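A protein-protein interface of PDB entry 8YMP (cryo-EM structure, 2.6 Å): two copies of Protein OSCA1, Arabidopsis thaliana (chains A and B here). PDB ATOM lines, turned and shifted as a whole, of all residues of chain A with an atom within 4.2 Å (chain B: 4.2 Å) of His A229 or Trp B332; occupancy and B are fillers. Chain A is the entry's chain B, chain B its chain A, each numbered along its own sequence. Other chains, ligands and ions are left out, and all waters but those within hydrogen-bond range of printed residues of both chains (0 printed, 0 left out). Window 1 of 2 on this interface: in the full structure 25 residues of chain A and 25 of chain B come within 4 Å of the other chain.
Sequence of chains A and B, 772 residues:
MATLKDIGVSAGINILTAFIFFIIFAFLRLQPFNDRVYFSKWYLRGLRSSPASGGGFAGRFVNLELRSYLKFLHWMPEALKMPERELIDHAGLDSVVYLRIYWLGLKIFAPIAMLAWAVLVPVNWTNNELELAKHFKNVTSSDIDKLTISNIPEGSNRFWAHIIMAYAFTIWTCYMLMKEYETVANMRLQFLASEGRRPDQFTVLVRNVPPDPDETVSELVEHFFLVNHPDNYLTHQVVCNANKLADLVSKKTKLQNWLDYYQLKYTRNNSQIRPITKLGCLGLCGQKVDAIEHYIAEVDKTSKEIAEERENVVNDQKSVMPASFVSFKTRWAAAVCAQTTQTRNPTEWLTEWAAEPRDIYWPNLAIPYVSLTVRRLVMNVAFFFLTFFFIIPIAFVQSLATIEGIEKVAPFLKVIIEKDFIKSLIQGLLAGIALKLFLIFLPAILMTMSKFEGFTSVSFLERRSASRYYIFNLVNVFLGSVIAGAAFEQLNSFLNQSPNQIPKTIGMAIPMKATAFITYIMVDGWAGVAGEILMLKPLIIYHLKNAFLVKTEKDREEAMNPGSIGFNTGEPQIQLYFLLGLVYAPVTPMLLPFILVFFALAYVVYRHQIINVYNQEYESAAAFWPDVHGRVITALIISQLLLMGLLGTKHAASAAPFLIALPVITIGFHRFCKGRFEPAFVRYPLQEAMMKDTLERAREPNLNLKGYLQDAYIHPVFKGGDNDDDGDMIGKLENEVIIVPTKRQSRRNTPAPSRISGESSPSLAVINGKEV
The backbone NH (N) of Trp B332 is in hydrogen-bond range of the side-chain carboxylate (OD2) of Asp B693, at 3.2 Å.
NE2 of His A229 is in hydrogen-bond range of SG of Cys A337.
The side-chain amide oxygen (OE1) of Gln A342 sits at hydrogen-bond distance from a ring nitrogen (NE2) of His A229 (2.8 Å).
NE2 of Gln A342 lies within hydrogen-bond range of O of Cys A337 (3.2 Å).
Of the printed residues of chain B, Asn A228 touches Trp B332 and Leu B686.
His A229 touches two residues of chain B.
Of the printed residues of chain B, Gln A342 touches Leu B686 (3.9 Å).
Trp B332 touches just these residues of chain A: Asn A228 and His A229.
Of the printed residues of chain A, Leu B686 touches Asn A228, His A229 and Gln A342.
The nearest printed residue of chain B that does not touch His A229 is Val B336 (5.9 Å).
The nearest printed residue of chain B that does not touch Gln A342 is Trp B332 (6.1 Å).
Among the printed residues, merely in contact across the chains: His A229 with Trp B332 (3.3 Å), Asn A228 with Leu B686 (3.6 Å), His A229 with Leu B686 (3.8 Å) and Gln A342 with Leu B686 (3.9 Å).
No position is printed for both chains.
Printed residues of chain B that touch a printed residue of chain A: Trp B332 and Leu B686.
Hydrophobic or aromatic side chains of chain B that line the printed part of chain A: Trp B332 and Leu B686.
Hydrophobic or aromatic side chains of chain A that line the printed part of chain B: His A229.
Among the printed residues, 5 pairs touch across the chains.
The indole nitrogen (NE1) of Trp B332 is in hydrogen-bond range of the backbone carbonyl oxygen (O) of Asn A228 (2.8 Å).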
ATOM      1  N   PHE A 225       8.050 -29.512 -17.880  1.00  0.00           N
ATOM      2  CA  PHE A 225       6.755 -28.885 -18.131  1.00  0.00           C
ATOM      3  C   PHE A 225       6.144 -28.135 -16.961  1.00  0.00           C
ATOM      4  O   PHE A 225       5.051 -27.609 -17.081  1.00  0.00           O
ATOM      5  CB  PHE A 225       5.772 -29.889 -18.713  1.00  0.00           C
ATOM      6  CG  PHE A 225       6.020 -30.195 -20.156  1.00  0.00           C
ATOM      7  CD1 PHE A 225       5.435 -29.430 -21.146  1.00  0.00           C
ATOM      8  CD2 PHE A 225       6.852 -31.235 -20.523  1.00  0.00           C
ATOM      9  CE1 PHE A 225       5.664 -29.703 -22.478  1.00  0.00           C
ATOM     10  CE2 PHE A 225       7.087 -31.514 -21.852  1.00  0.00           C
ATOM     11  CZ  PHE A 225       6.492 -30.746 -22.832  1.00  0.00           C
ATOM     12  N   VAL A 227       8.195 -25.930 -15.391  1.00  0.00           N
ATOM     13  CA  VAL A 227       8.949 -24.699 -15.450  1.00  0.00           C
ATOM     14  C   VAL A 227       8.707 -24.003 -16.774  1.00  0.00           C
ATOM     15  O   VAL A 227       8.889 -22.795 -16.878  1.00  0.00           O
ATOM     16  CB  VAL A 227      10.455 -24.924 -15.220  1.00  0.00           C
ATOM     17  CG1 VAL A 227      10.693 -25.630 -13.896  1.00  0.00           C
ATOM     18  CG2 VAL A 227      11.093 -25.692 -16.362  1.00  0.00           C
ATOM     19  N   ASN A 228       8.273 -24.750 -17.782  1.00  0.00           N
ATOM     20  CA  ASN A 228       8.039 -24.164 -19.090  1.00  0.00           C
ATOM     21  C   ASN A 228       6.585 -23.780 -19.275  1.00  0.00           C
ATOM     22  O   ASN A 228       6.301 -22.714 -19.809  1.00  0.00           O
ATOM     23  CB  ASN A 228       8.495 -25.101 -20.196  1.00  0.00           C
ATOM     24  CG  ASN A 228       9.978 -24.996 -20.469  1.00  0.00           C
ATOM     25  OD1 ASN A 228      10.799 -25.415 -19.659  1.00  0.00           O
ATOM     26  ND2 ASN A 228      10.329 -24.434 -21.617  1.00  0.00           N
ATOM     27  N   HIS A 229       5.659 -24.629 -18.848  1.00  0.00           N
ATOM     28  CA  HIS A 229       4.236 -24.292 -18.910  1.00  0.00           C
ATOM     29  C   HIS A 229       3.735 -24.375 -17.495  1.00  0.00           C
ATOM     30  O   HIS A 229       3.058 -25.326 -17.140  1.00  0.00           O
ATOM     31  CB  HIS A 229       3.482 -25.285 -19.780  1.00  0.00           C
ATOM     32  CG  HIS A 229       3.923 -25.296 -21.209  1.00  0.00           C
ATOM     33  ND1 HIS A 229       3.253 -24.613 -22.198  1.00  0.00           N
ATOM     34  CD2 HIS A 229       4.966 -25.909 -21.815  1.00  0.00           C
ATOM     35  CE1 HIS A 229       3.866 -24.800 -23.352  1.00  0.00           C
ATOM     36  NE2 HIS A 229       4.908 -25.584 -23.147  1.00  0.00           N
ATOM     37  N   PRO A 230       4.028 -23.362 -16.678  1.00  0.00           N
ATOM     38  CA  PRO A 230       3.699 -23.474 -15.255  1.00  0.00           C
ATOM     39  C   PRO A 230       2.240 -23.457 -14.843  1.00  0.00           C
ATOM     40  O   PRO A 230       1.851 -24.303 -14.045  1.00  0.00           O
ATOM     41  CB  PRO A 230       4.414 -22.259 -14.642  1.00  0.00           C
ATOM     42  CG  PRO A 230       5.192 -21.612 -15.745  1.00  0.00           C
ATOM     43  CD  PRO A 230       4.520 -22.020 -17.014  1.00  0.00           C
ATOM     44  N   ASP A 231       1.445 -22.528 -15.348  1.00  0.00           N
ATOM     45  CA  ASP A 231       0.064 -22.394 -14.883  1.00  0.00           C
ATOM     46  C   ASP A 231      -0.950 -23.308 -15.530  1.00  0.00           C
ATOM     47  O   ASP A 231      -2.131 -23.235 -15.214  1.00  0.00           O
ATOM     48  CB  ASP A 231      -0.394 -20.950 -15.065  1.00  0.00           C
ATOM     49  CG  ASP A 231       0.479 -20.182 -16.036  1.00  0.00           C
ATOM     50  OD1 ASP A 231       0.468 -20.514 -17.240  1.00  0.00           O
ATOM     51  OD2 ASP A 231       1.176 -19.244 -15.596  1.00  0.00           O
ATOM     52  N   ASN A 232      -0.511 -24.170 -16.430  1.00  0.00           N
ATOM     53  CA  ASN A 232      -1.459 -24.999 -17.139  1.00  0.00           C
ATOM     54  C   ASN A 232      -1.128 -26.482 -17.115  1.00  0.00           C
ATOM     55  O   ASN A 232      -2.000 -27.308 -17.328  1.00  0.00           O
ATOM     56  CB  ASN A 232      -1.586 -24.510 -18.567  1.00  0.00           C
ATOM     57  CG  ASN A 232      -2.307 -23.183 -18.661  1.00  0.00           C
ATOM     58  OD1 ASN A 232      -3.469 -23.067 -18.275  1.00  0.00           O
ATOM     59  ND2 ASN A 232      -1.620 -22.171 -19.180  1.00  0.00           N
ATOM     60  N   TYR A 233       0.120 -26.827 -16.849  1.00  0.00           N
ATOM     61  CA  TYR A 233       0.512 -28.224 -16.803  1.00  0.00           C
ATOM     62  C   TYR A 233      -0.291 -28.943 -15.758  1.00  0.00           C
ATOM     63  O   TYR A 233      -0.342 -28.518 -14.611  1.00  0.00           O
ATOM     64  CB  TYR A 233       1.993 -28.329 -16.484  1.00  0.00           C
ATOM     65  CG  TYR A 233       2.517 -29.718 -16.218  1.00  0.00           C
ATOM     66  CD1 TYR A 233       2.382 -30.729 -17.154  1.00  0.00           C
ATOM     67  CD2 TYR A 233       3.174 -30.008 -15.035  1.00  0.00           C
ATOM     68  CE1 TYR A 233       2.874 -31.994 -16.909  1.00  0.00           C
ATOM     69  CE2 TYR A 233       3.670 -31.266 -14.782  1.00  0.00           C
ATOM     70  CZ  TYR A 233       3.517 -32.253 -15.722  1.00  0.00           C
ATOM     71  OH  TYR A 233       4.014 -33.503 -15.466  1.00  0.00           O
ATOM     72  N   PHE A 328      -2.831 -30.780 -20.279  1.00  0.00           N
ATOM     73  CA  PHE A 328      -2.956 -29.437 -19.729  1.00  0.00           C
ATOM     74  C   PHE A 328      -4.348 -29.141 -19.208  1.00  0.00           C
ATOM     75  O   PHE A 328      -5.289 -29.868 -19.495  1.00  0.00           O
ATOM     76  CB  PHE A 328      -2.548 -28.402 -20.775  1.00  0.00           C
ATOM     77  CG  PHE A 328      -1.117 -28.504 -21.193  1.00  0.00           C
ATOM     78  CD1 PHE A 328      -0.133 -27.850 -20.484  1.00  0.00           C
ATOM     79  CD2 PHE A 328      -0.755 -29.259 -22.291  1.00  0.00           C
ATOM     80  CE1 PHE A 328       1.189 -27.944 -20.859  1.00  0.00           C
ATOM     81  CE2 PHE A 328       0.563 -29.359 -22.671  1.00  0.00           C
ATOM     82  CZ  PHE A 328       1.538 -28.699 -21.955  1.00  0.00           C
ATOM     83  N   CYS A 337       0.998 -25.277 -26.506  1.00  0.00           N
ATOM     84  CA  CYS A 337       2.104 -26.227 -26.498  1.00  0.00           C
ATOM     85  C   CYS A 337       2.275 -26.956 -27.817  1.00  0.00           C
ATOM     86  O   CYS A 337       3.394 -27.224 -28.234  1.00  0.00           O
ATOM     87  CB  CYS A 337       1.942 -27.237 -25.374  1.00  0.00           C
ATOM     88  SG  CYS A 337       3.409 -28.232 -25.061  1.00  0.00           S
ATOM     89  N   GLN A 342       9.650 -26.027 -28.161  1.00  0.00           N
ATOM     90  CA  GLN A 342       9.917 -26.100 -26.731  1.00  0.00           C
ATOM     91  C   GLN A 342      11.357 -25.911 -26.280  1.00  0.00           C
ATOM     92  O   GLN A 342      11.587 -25.367 -25.204  1.00  0.00           O
ATOM     93  CB  GLN A 342       9.362 -27.400 -26.167  1.00  0.00           C
ATOM     94  CG  GLN A 342       7.918 -27.657 -26.540  1.00  0.00           C
ATOM     95  CD  GLN A 342       6.967 -26.736 -25.814  1.00  0.00           C
ATOM     96  OE1 GLN A 342       7.133 -26.471 -24.626  1.00  0.00           O
ATOM     97  NE2 GLN A 342       5.963 -26.244 -26.525  1.00  0.00           N
ATOM     98  N   THR B 330       5.067 -11.391 -20.280  1.00  0.00           N
ATOM     99  CA  THR B 330       6.235 -12.252 -20.302  1.00  0.00           C
ATOM    100  C   THR B 330       6.755 -12.538 -21.693  1.00  0.00           C
ATOM    101  O   THR B 330       6.019 -12.435 -22.666  1.00  0.00           O
ATOM    102  CB  THR B 330       5.923 -13.591 -19.622  1.00  0.00           C
ATOM    103  OG1 THR B 330       4.504 -13.758 -19.523  1.00  0.00           O
ATOM    104  CG2 THR B 330       6.525 -13.634 -18.233  1.00  0.00           C
ATOM    105  N   ARG B 331       8.029 -12.891 -21.794  1.00  0.00           N
ATOM    106  CA  ARG B 331       8.602 -13.262 -23.078  1.00  0.00           C
ATOM    107  C   ARG B 331       7.909 -14.525 -23.527  1.00  0.00           C
ATOM    108  O   ARG B 331       7.561 -14.659 -24.694  1.00  0.00           O
ATOM    109  CB  ARG B 331      10.100 -13.528 -22.919  1.00  0.00           C
ATOM    110  CG  ARG B 331      11.000 -12.539 -23.628  1.00  0.00           C
ATOM    111  CD  ARG B 331      12.375 -12.506 -22.993  1.00  0.00           C
ATOM    112  NE  ARG B 331      12.302 -12.275 -21.557  1.00  0.00           N
ATOM    113  CZ  ARG B 331      12.962 -11.315 -20.922  1.00  0.00           C
ATOM    114  NH1 ARG B 331      13.749 -10.492 -21.597  1.00  0.00           N
ATOM    115  NH2 ARG B 331      12.836 -11.176 -19.612  1.00  0.00           N
ATOM    116  N   TRP B 332       7.697 -15.452 -22.603  1.00  0.00           N
ATOM    117  CA  TRP B 332       7.026 -16.702 -22.910  1.00  0.00           C
ATOM    118  C   TRP B 332       5.680 -16.454 -23.548  1.00  0.00           C
ATOM    119  O   TRP B 332       5.350 -17.073 -24.549  1.00  0.00           O
ATOM    120  CB  TRP B 332       6.854 -17.496 -21.615  1.00  0.00           C
ATOM    121  CG  TRP B 332       6.288 -18.863 -21.762  1.00  0.00           C
ATOM    122  CD1 TRP B 332       6.982 -20.017 -21.942  1.00  0.00           C
ATOM    123  CD2 TRP B 332       4.905 -19.230 -21.706  1.00  0.00           C
ATOM    124  NE1 TRP B 332       6.120 -21.080 -22.018  1.00  0.00           N
ATOM    125  CE2 TRP B 332       4.837 -20.622 -21.878  1.00  0.00           C
ATOM    126  CE3 TRP B 332       3.718 -18.513 -21.536  1.00  0.00           C
ATOM    127  CZ2 TRP B 332       3.631 -21.312 -21.885  1.00  0.00           C
ATOM    128  CZ3 TRP B 332       2.525 -19.199 -21.545  1.00  0.00           C
ATOM    129  CH2 TRP B 332       2.489 -20.584 -21.718  1.00  0.00           C
ATOM    130  N   ALA B 333       4.899 -15.545 -22.982  1.00  0.00           N
ATOM    131  CA  ALA B 333       3.558 -15.292 -23.492  1.00  0.00           C
ATOM    132  C   ALA B 333       3.532 -14.713 -24.884  1.00  0.00           C
ATOM    133  O   ALA B 333       2.687 -15.073 -25.690  1.00  0.00           O
ATOM    134  CB  ALA B 333       2.830 -14.371 -22.557  1.00  0.00           C
ATOM    135  N   ALA B 334       4.443 -13.799 -25.169  1.00  0.00           N
ATOM    136  CA  ALA B 334       4.493 -13.185 -26.478  1.00  0.00           C
ATOM    137  C   ALA B 334       4.918 -14.213 -27.478  1.00  0.00           C
ATOM    138  O   ALA B 334       4.423 -14.230 -28.593  1.00  0.00           O
ATOM    139  CB  ALA B 334       5.463 -12.037 -26.473  1.00  0.00           C
ATOM    140  N   ALA B 335       5.845 -15.078 -27.088  1.00  0.00           N
ATOM    141  CA  ALA B 335       6.278 -16.144 -27.965  1.00  0.00           C
ATOM    142  C   ALA B 335       5.085 -16.991 -28.315  1.00  0.00           C
ATOM    143  O   ALA B 335       4.874 -17.297 -29.475  1.00  0.00           O
ATOM    144  CB  ALA B 335       7.349 -16.971 -27.303  1.00  0.00           C
ATOM    145  N   VAL B 336       4.281 -17.352 -27.325  1.00  0.00           N
ATOM    146  CA  VAL B 336       3.063 -18.101 -27.600  1.00  0.00           C
ATOM    147  C   VAL B 336       2.213 -17.380 -28.640  1.00  0.00           C
ATOM    148  O   VAL B 336       1.914 -17.941 -29.685  1.00  0.00           O
ATOM    149  CB  VAL B 336       2.251 -18.356 -26.320  1.00  0.00           C
ATOM    150  CG1 VAL B 336       0.868 -18.890 -26.651  1.00  0.00           C
ATOM    151  CG2 VAL B 336       2.991 -19.327 -25.419  1.00  0.00           C
ATOM    152  N   LEU B 686      10.366 -21.843 -26.337  1.00  0.00           N
ATOM    153  CA  LEU B 686       9.609 -21.426 -25.164  1.00  0.00           C
ATOM    154  C   LEU B 686      10.418 -21.637 -23.894  1.00  0.00           C
ATOM    155  O   LEU B 686      10.271 -20.890 -22.933  1.00  0.00           O
ATOM    156  CB  LEU B 686       8.281 -22.179 -25.086  1.00  0.00           C
ATOM    157  CG  LEU B 686       6.998 -21.411 -25.393  1.00  0.00           C
ATOM    158  CD1 LEU B 686       7.118 -20.642 -26.693  1.00  0.00           C
ATOM    159  CD2 LEU B 686       5.820 -22.368 -25.449  1.00  0.00           C
ATOM    160  N   ALA B 689      12.758 -18.730 -23.418  1.00  0.00           N
ATOM    161  CA  ALA B 689      12.016 -17.571 -22.959  1.00  0.00           C
ATOM    162  C   ALA B 689      11.778 -17.661 -21.472  1.00  0.00           C
ATOM    163  O   ALA B 689      11.996 -16.700 -20.751  1.00  0.00           O
ATOM    164  CB  ALA B 689      10.699 -17.472 -23.692  1.00  0.00           C
ATOM    165  N   ASP B 693      13.120 -15.124 -18.572  1.00  0.00           N
ATOM    166  CA  ASP B 693      12.172 -14.483 -17.683  1.00  0.00           C
ATOM    167  C   ASP B 693      12.519 -14.733 -16.237  1.00  0.00           C
ATOM    168  O   ASP B 693      12.623 -13.798 -15.461  1.00  0.00           O
ATOM    169  CB  ASP B 693      10.768 -15.000 -17.961  1.00  0.00           C
ATOM    170  CG  ASP B 693      10.161 -14.402 -19.205  1.00  0.00           C
ATOM    171  OD1 ASP B 693      10.388 -13.204 -19.461  1.00  0.00           O
ATOM    172  OD2 ASP B 693       9.451 -15.132 -19.922  1.00  0.00           O
